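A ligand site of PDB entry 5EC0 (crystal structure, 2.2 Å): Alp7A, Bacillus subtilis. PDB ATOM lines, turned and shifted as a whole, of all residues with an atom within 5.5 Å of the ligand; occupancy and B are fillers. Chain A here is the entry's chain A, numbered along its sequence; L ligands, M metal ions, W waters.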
ATOM      1  N   GLY A  11      15.209  13.242  31.506  1.00  0.00           N
ATOM      2  CA  GLY A  11      13.904  12.706  31.168  1.00  0.00           C
ATOM      3  C   GLY A  11      13.830  11.198  31.347  1.00  0.00           C
ATOM      4  O   GLY A  11      14.849  10.547  31.577  1.00  0.00           O
ATOM      5  N   ASN A  12      12.629  10.651  31.245  1.00  0.00           N
ATOM      6  CA  ASN A  12      12.450   9.208  31.303  1.00  0.00           C
ATOM      7  C   ASN A  12      12.751   8.594  29.932  1.00  0.00           C
ATOM      8  O   ASN A  12      13.152   7.441  29.846  1.00  0.00           O
ATOM      9  CB  ASN A  12      11.017   8.844  31.730  1.00  0.00           C
ATOM     10  CG  ASN A  12      10.572   9.579  32.991  1.00  0.00           C
ATOM     11  OD1 ASN A  12      11.323   9.681  33.968  1.00  0.00           O
ATOM     12  ND2 ASN A  12       9.348  10.086  32.976  1.00  0.00           N
ATOM     13  N   SER A  13      12.562   9.391  28.882  1.00  0.00           N
ATOM     14  CA  SER A  13      12.741   8.929  27.510  1.00  0.00           C
ATOM     15  C   SER A  13      14.102   9.354  26.949  1.00  0.00           C
ATOM     16  O   SER A  13      14.835   8.541  26.387  1.00  0.00           O
ATOM     17  CB  SER A  13      11.621   9.448  26.617  1.00  0.00           C
ATOM     18  OG  SER A  13      11.848   9.155  25.254  1.00  0.00           O
ATOM     19  N   MET A  14      14.412  10.623  27.132  1.00  0.00           N
ATOM     20  CA  MET A  14      15.674  11.196  26.686  1.00  0.00           C
ATOM     21  C   MET A  14      16.317  12.010  27.803  1.00  0.00           C
ATOM     22  O   MET A  14      15.648  12.766  28.488  1.00  0.00           O
ATOM     23  CB  MET A  14      15.467  12.091  25.444  1.00  0.00           C
ATOM     24  CG  MET A  14      14.918  11.405  24.195  1.00  0.00           C
ATOM     25  SD  MET A  14      15.979  10.128  23.463  1.00  0.00           S
ATOM     26  CE  MET A  14      17.315  11.117  22.823  1.00  0.00           C
ATOM     27  N   GLU A  25      21.086  15.302  22.817  1.00  0.00           N
ATOM     28  CA  GLU A  25      20.344  14.408  23.692  1.00  0.00           C
ATOM     29  C   GLU A  25      20.776  12.960  23.458  1.00  0.00           C
ATOM     30  O   GLU A  25      21.367  12.637  22.446  1.00  0.00           O
ATOM     31  CB  GLU A  25      18.839  14.565  23.476  1.00  0.00           C
ATOM     32  CG  GLU A  25      18.384  14.549  22.029  1.00  0.00           C
ATOM     33  CD  GLU A  25      16.865  14.639  21.887  1.00  0.00           C
ATOM     34  OE1 GLU A  25      16.168  14.427  22.889  1.00  0.00           O
ATOM     35  OE2 GLU A  25      16.359  14.921  20.777  1.00  0.00           O
ATOM     36  N   ASP A 212       2.489  19.410  31.797  1.00  0.00           N
ATOM     37  CA  ASP A 212       3.683  18.736  31.309  1.00  0.00           C
ATOM     38  C   ASP A 212       3.352  17.281  30.970  1.00  0.00           C
ATOM     39  O   ASP A 212       3.409  16.398  31.841  1.00  0.00           O
ATOM     40  CB  ASP A 212       4.793  18.830  32.367  1.00  0.00           C
ATOM     41  CG  ASP A 212       6.156  18.364  31.858  1.00  0.00           C
ATOM     42  OD1 ASP A 212       6.242  17.750  30.767  1.00  0.00           O
ATOM     43  OD2 ASP A 212       7.142  18.588  32.585  1.00  0.00           O
ATOM     44  N   LEU A 213       2.982  17.026  29.719  1.00  0.00           N
ATOM     45  CA  LEU A 213       2.548  15.687  29.330  1.00  0.00           C
ATOM     46  C   LEU A 213       3.727  14.878  28.813  1.00  0.00           C
ATOM     47  O   LEU A 213       4.252  15.166  27.738  1.00  0.00           O
ATOM     48  CB  LEU A 213       1.446  15.753  28.252  1.00  0.00           C
ATOM     49  CG  LEU A 213       0.269  16.720  28.497  1.00  0.00           C
ATOM     50  CD1 LEU A 213      -0.691  16.795  27.285  1.00  0.00           C
ATOM     51  CD2 LEU A 213      -0.497  16.379  29.762  1.00  0.00           C
ATOM     52  N   GLY A 214       4.127  13.850  29.560  1.00  0.00           N
ATOM     53  CA  GLY A 214       5.265  13.024  29.196  1.00  0.00           C
ATOM     54  C   GLY A 214       4.911  11.591  28.863  1.00  0.00           C
ATOM     55  O   GLY A 214       3.745  11.198  28.913  1.00  0.00           O
ATOM     56  N   GLY A 215       5.928  10.801  28.537  1.00  0.00           N
ATOM     57  CA  GLY A 215       5.752   9.386  28.217  1.00  0.00           C
ATOM     58  C   GLY A 215       5.302   8.587  29.418  1.00  0.00           C
ATOM     59  O   GLY A 215       4.464   7.699  29.279  1.00  0.00           O
ATOM     60  N   GLY A 216       5.830   8.899  30.604  1.00  0.00           N
ATOM     61  CA  GLY A 216       5.543   8.094  31.776  1.00  0.00           C
ATOM     62  C   GLY A 216       4.761   8.757  32.889  1.00  0.00           C
ATOM     63  O   GLY A 216       4.192   8.082  33.754  1.00  0.00           O
ATOM     64  N   THR A 217       4.721  10.090  32.891  1.00  0.00           N
ATOM     65  CA  THR A 217       3.901  10.854  33.843  1.00  0.00           C
ATOM     66  C   THR A 217       3.245  12.054  33.172  1.00  0.00           C
ATOM     67  O   THR A 217       3.682  12.515  32.109  1.00  0.00           O
ATOM     68  CB  THR A 217       4.714  11.390  35.052  1.00  0.00           C
ATOM     69  OG1 THR A 217       5.652  12.368  34.614  1.00  0.00           O
ATOM     70  CG2 THR A 217       5.449  10.269  35.786  1.00  0.00           C
ATOM     71  N   PHE A 243       1.205   7.344  29.016  1.00  0.00           N
ATOM     72  CA  PHE A 243       1.096   7.322  27.562  1.00  0.00           C
ATOM     73  C   PHE A 243       1.714   6.064  26.939  1.00  0.00           C
ATOM     74  O   PHE A 243       1.177   5.504  25.972  1.00  0.00           O
ATOM     75  CB  PHE A 243       1.772   8.565  26.989  1.00  0.00           C
ATOM     76  CG  PHE A 243       1.771   8.630  25.495  1.00  0.00           C
ATOM     77  CD1 PHE A 243       0.590   8.768  24.791  1.00  0.00           C
ATOM     78  CD2 PHE A 243       2.970   8.580  24.806  1.00  0.00           C
ATOM     79  CE1 PHE A 243       0.602   8.849  23.416  1.00  0.00           C
ATOM     80  CE2 PHE A 243       2.987   8.661  23.419  1.00  0.00           C
ATOM     81  CZ  PHE A 243       1.801   8.799  22.727  1.00  0.00           C
ATOM     82  N   LEU A 244       2.842   5.614  27.483  1.00  0.00           N
ATOM     83  CA  LEU A 244       3.520   4.439  26.955  1.00  0.00           C
ATOM     84  C   LEU A 244       2.675   3.175  27.103  1.00  0.00           C
ATOM     85  O   LEU A 244       2.684   2.304  26.228  1.00  0.00           O
ATOM     86  CB  LEU A 244       4.869   4.245  27.636  1.00  0.00           C
ATOM     87  CG  LEU A 244       5.919   5.253  27.170  1.00  0.00           C
ATOM     88  CD1 LEU A 244       7.165   5.166  28.025  1.00  0.00           C
ATOM     89  CD2 LEU A 244       6.260   5.028  25.705  1.00  0.00           C
ATOM     90  N   GLU A 266       6.291   4.307  19.192  1.00  0.00           N
ATOM     91  CA  GLU A 266       6.576   5.641  19.703  1.00  0.00           C
ATOM     92  C   GLU A 266       7.419   6.472  18.731  1.00  0.00           C
ATOM     93  O   GLU A 266       7.108   7.628  18.497  1.00  0.00           O
ATOM     94  CB  GLU A 266       7.270   5.515  21.060  1.00  0.00           C
ATOM     95  CG  GLU A 266       7.691   6.827  21.712  1.00  0.00           C
ATOM     96  CD  GLU A 266       8.579   6.577  22.918  1.00  0.00           C
ATOM     97  OE1 GLU A 266       9.458   5.676  22.837  1.00  0.00           O
ATOM     98  OE2 GLU A 266       8.417   7.270  23.937  1.00  0.00           O
ATOM     99  N   TYR A 270       6.017  10.097  16.615  1.00  0.00           N
ATOM    100  CA  TYR A 270       6.511  11.485  16.641  1.00  0.00           C
ATOM    101  C   TYR A 270       7.249  11.844  15.347  1.00  0.00           C
ATOM    102  O   TYR A 270       7.184  12.979  14.902  1.00  0.00           O
ATOM    103  CB  TYR A 270       7.407  11.774  17.878  1.00  0.00           C
ATOM    104  CG  TYR A 270       8.761  11.094  17.959  1.00  0.00           C
ATOM    105  CD1 TYR A 270       9.853  11.549  17.206  1.00  0.00           C
ATOM    106  CD2 TYR A 270       8.984  10.054  18.860  1.00  0.00           C
ATOM    107  CE1 TYR A 270      11.116  10.944  17.310  1.00  0.00           C
ATOM    108  CE2 TYR A 270      10.246   9.442  18.971  1.00  0.00           C
ATOM    109  CZ  TYR A 270      11.292   9.894  18.195  1.00  0.00           C
ATOM    110  OH  TYR A 270      12.519   9.278  18.328  1.00  0.00           O
ATOM    111  N   GLY A 328       5.679  19.242  27.101  1.00  0.00           N
ATOM    112  CA  GLY A 328       6.219  17.894  27.147  1.00  0.00           C
ATOM    113  C   GLY A 328       6.215  17.282  25.755  1.00  0.00           C
ATOM    114  O   GLY A 328       5.588  17.823  24.830  1.00  0.00           O
ATOM    115  N   GLY A 329       6.905  16.152  25.612  1.00  0.00           N
ATOM    116  CA  GLY A 329       7.049  15.474  24.330  1.00  0.00           C
ATOM    117  C   GLY A 329       5.739  14.870  23.831  1.00  0.00           C
ATOM    118  O   GLY A 329       5.478  14.816  22.631  1.00  0.00           O
ATOM    119  N   VAL A 330       4.914  14.411  24.760  1.00  0.00           N
ATOM    120  CA  VAL A 330       3.602  13.898  24.374  1.00  0.00           C
ATOM    121  C   VAL A 330       2.678  15.057  23.977  1.00  0.00           C
ATOM    122  O   VAL A 330       1.842  14.895  23.086  1.00  0.00           O
ATOM    123  CB  VAL A 330       2.986  13.050  25.516  1.00  0.00           C
ATOM    124  CG1 VAL A 330       1.544  12.655  25.193  1.00  0.00           C
ATOM    125  CG2 VAL A 330       3.833  11.795  25.729  1.00  0.00           C
ATOM    126  N   GLU A 332       3.445  17.777  22.450  1.00  0.00           N
ATOM    127  CA  GLU A 332       3.867  18.033  21.080  1.00  0.00           C
ATOM    128  C   GLU A 332       3.178  17.085  20.078  1.00  0.00           C
ATOM    129  O   GLU A 332       2.693  17.508  19.047  1.00  0.00           O
ATOM    130  CB  GLU A 332       5.392  17.880  20.994  1.00  0.00           C
ATOM    131  CG  GLU A 332       6.013  18.378  19.702  1.00  0.00           C
ATOM    132  CD  GLU A 332       7.539  18.482  19.801  1.00  0.00           C
ATOM    133  OE1 GLU A 332       8.225  17.696  19.129  1.00  0.00           O
ATOM    134  OE2 GLU A 332       8.051  19.368  20.554  1.00  0.00           O
ATOM    135  N   VAL A 333       3.127  15.802  20.425  1.00  0.00           N
ATOM    136  CA  VAL A 333       2.524  14.786  19.580  1.00  0.00           C
ATOM    137  C   VAL A 333       0.995  14.947  19.513  1.00  0.00           C
ATOM    138  O   VAL A 333       0.367  14.768  18.456  1.00  0.00           O
ATOM    139  CB  VAL A 333       2.884  13.388  20.120  1.00  0.00           C
ATOM    140  CG1 VAL A 333       1.968  12.315  19.556  1.00  0.00           C
ATOM    141  CG2 VAL A 333       4.360  13.078  19.819  1.00  0.00           C
ATOM    142  N   ARG A 362       8.426  19.943  23.736  1.00  0.00           N
ATOM    143  CA  ARG A 362       9.319  18.929  24.282  1.00  0.00           C
ATOM    144  C   ARG A 362      10.514  19.532  25.056  1.00  0.00           C
ATOM    145  O   ARG A 362      11.008  18.931  26.003  1.00  0.00           O
ATOM    146  CB  ARG A 362       9.840  18.002  23.178  1.00  0.00           C
ATOM    147  CG  ARG A 362      10.499  16.755  23.725  1.00  0.00           C
ATOM    148  CD  ARG A 362      10.678  15.662  22.637  1.00  0.00           C
ATOM    149  NE  ARG A 362      11.664  16.020  21.621  1.00  0.00           N
ATOM    150  CZ  ARG A 362      12.955  15.654  21.675  1.00  0.00           C
ATOM    151  NH1 ARG A 362      13.379  14.928  22.686  1.00  0.00           N
ATOM    152  NH2 ARG A 362      13.800  16.012  20.715  1.00  0.00           N
HETATM  153  P1  LIG L   1       9.290  11.557  29.529  1.00  0.00           P
HETATM  154  O1  LIG L   1      10.554  12.276  29.982  1.00  0.00           O
HETATM  155  O2  LIG L   1       8.363  11.091  30.628  1.00  0.00           O
HETATM  156  O3  LIG L   1       9.476  10.485  28.478  1.00  0.00           O
HETATM  157  P2  LIG L   1       8.980  13.611  27.498  1.00  0.00           P
HETATM  158  O4  LIG L   1      10.455  13.388  27.245  1.00  0.00           O
HETATM  159  O5  LIG L   1       8.429  15.015  27.627  1.00  0.00           O
HETATM  160  O6  LIG L   1       8.465  12.717  28.752  1.00  0.00           O
HETATM  161  O7  LIG L   1       8.154  12.873  26.350  1.00  0.00           O
HETATM  162  C1  LIG L   1       8.662  11.755  25.627  1.00  0.00           C
HETATM  163  C2  LIG L   1       7.746  11.643  24.429  1.00  0.00           C
HETATM  164  O8  LIG L   1       8.072  12.688  23.515  1.00  0.00           O
HETATM  165  C3  LIG L   1       7.888  10.353  23.638  1.00  0.00           C
HETATM  166  O9  LIG L   1       6.873   9.417  24.010  1.00  0.00           O
HETATM  167  C4  LIG L   1       7.694  10.776  22.190  1.00  0.00           C
HETATM  168  O10 LIG L   1       6.435  10.262  21.751  1.00  0.00           O
HETATM  169  C5  LIG L   1       7.644  12.303  22.222  1.00  0.00           C
HETATM  170  N1  LIG L   1       8.508  12.957  21.211  1.00  0.00           N
HETATM  171  C6  LIG L   1       8.078  13.963  20.424  1.00  0.00           C
HETATM  172  N2  LIG L   1       9.058  14.397  19.604  1.00  0.00           N
HETATM  173  C7  LIG L   1      10.158  13.665  19.876  1.00  0.00           C
HETATM  174  C8  LIG L   1      11.526  13.637  19.347  1.00  0.00           C
HETATM  175  N3  LIG L   1      11.891  14.500  18.364  1.00  0.00           N
HETATM  176  N4  LIG L   1      12.391  12.740  19.882  1.00  0.00           N
HETATM  177  C9  LIG L   1      11.999  11.889  20.860  1.00  0.00           C
HETATM  178  N5  LIG L   1      10.756  11.850  21.407  1.00  0.00           N
HETATM  179  C10 LIG L   1       9.796  12.705  20.947  1.00  0.00           C
HETATM  180 MG    MG M   1       9.941  15.732  31.191  1.00  0.00          MG
HETATM  181  O   HOH W   1      11.028  14.665  29.733  1.00  0.00           O
HETATM  182  O   HOH W   2       9.607  13.942  31.959  1.00  0.00           O
HETATM  183  O   HOH W   3      10.182  16.998  27.813  1.00  0.00           O
HETATM  184  O   HOH W   4       7.935  15.452  30.159  1.00  0.00           O
HETATM  185  O   HOH W   5      12.439  12.213  28.344  1.00  0.00           O
HETATM  186  O   HOH W   6      11.875  13.510  24.603  1.00  0.00           O
HETATM  187  O   HOH W   7      15.010  12.753  19.337  1.00  0.00           O
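N of Phe 243 sits at hydrogen-bond distance from O of Gly 215 (3.3 Å).
OE2 of Glu 25 is in salt-bridge range of NH2 of Arg 362.
The backbone NH of Val 330 is in hydrogen-bond range of the backbone carbonyl oxygen of Leu 213, at 3.1 Å.
O of Gly 215 lies within hydrogen-bond range of N of Leu 244, at 3.2 Å.
OE2 of Glu 332 lies within hydrogen-bond range of N of Arg 362.
Water W4 bridges O5 of the ligand and OD1 of Asp 212.
Water W3 bridges an oxygen (O5) of the ligand and the backbone carbonyl oxygen of Arg 362.
Water W7 lies within hydrogen-bond range of a nitrogen (N4) of the ligand (2.7 Å) and the side-chain carboxylate of Glu 25 (2.9 Å).
Water W6 bridges NH1 of Arg 362 (2.8 Å) and O4 of the ligand (3.0 Å).
OE1 of Glu 332 sits close to N2 of the ligand, at 3.4 Å.
The guanidinium group (NH2) of Arg 362 sits close to a nitrogen (N3) of the ligand (3.4 Å).
Gly 11 touches the ligand (CA to O1, 3.6 Å).
CA of Gly 214 touches O6 of the ligand, at 3.2 Å.
Tyr 270 touches the ligand (CE1 to N4, 3.4 Å).
CA of Gly 328 touches O5 of the ligand, at 3.7 Å.
Val 330 touches the ligand.
CG2 of Val 333 touches C6 of the ligand, at 3.9 Å.
Within 4 Å of the ligand: Gly 11, Asn 12, Ser 13, Gly 214, Gly 215, Gly 216, Glu 266, Tyr 270, Gly 328, Gly 329, Val 330, Glu 332, Val 333 and Arg 362.
The nearest printed residue that does not touch the ligand is Phe 243 (4.003 Å).
O1 of the ligand is in hydrogen-bond range of N of Asn 12, 2.9 Å away.
An oxygen (O6) of the ligand sits at hydrogen-bond distance from the backbone NH (N) of Gly 215.
An oxygen (O3) of the ligand lies close to the backbone NH of Ser 13, 3.3 Å away.
O2 of the ligand sits at hydrogen-bond distance from N of Gly 216 (3.3 Å).
ND2 of Asn 12 lies within hydrogen-bond range of O2 of the ligand, at 2.7 Å.
The side-chain carboxylate (OE2) of Glu 266 is in hydrogen-bond range of an oxygen (O9) of the ligand, at 2.6 Å.
The backbone NH (N) of Gly 329 lies within hydrogen-bond range of an oxygen (O5) of the ligand (2.8 Å).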
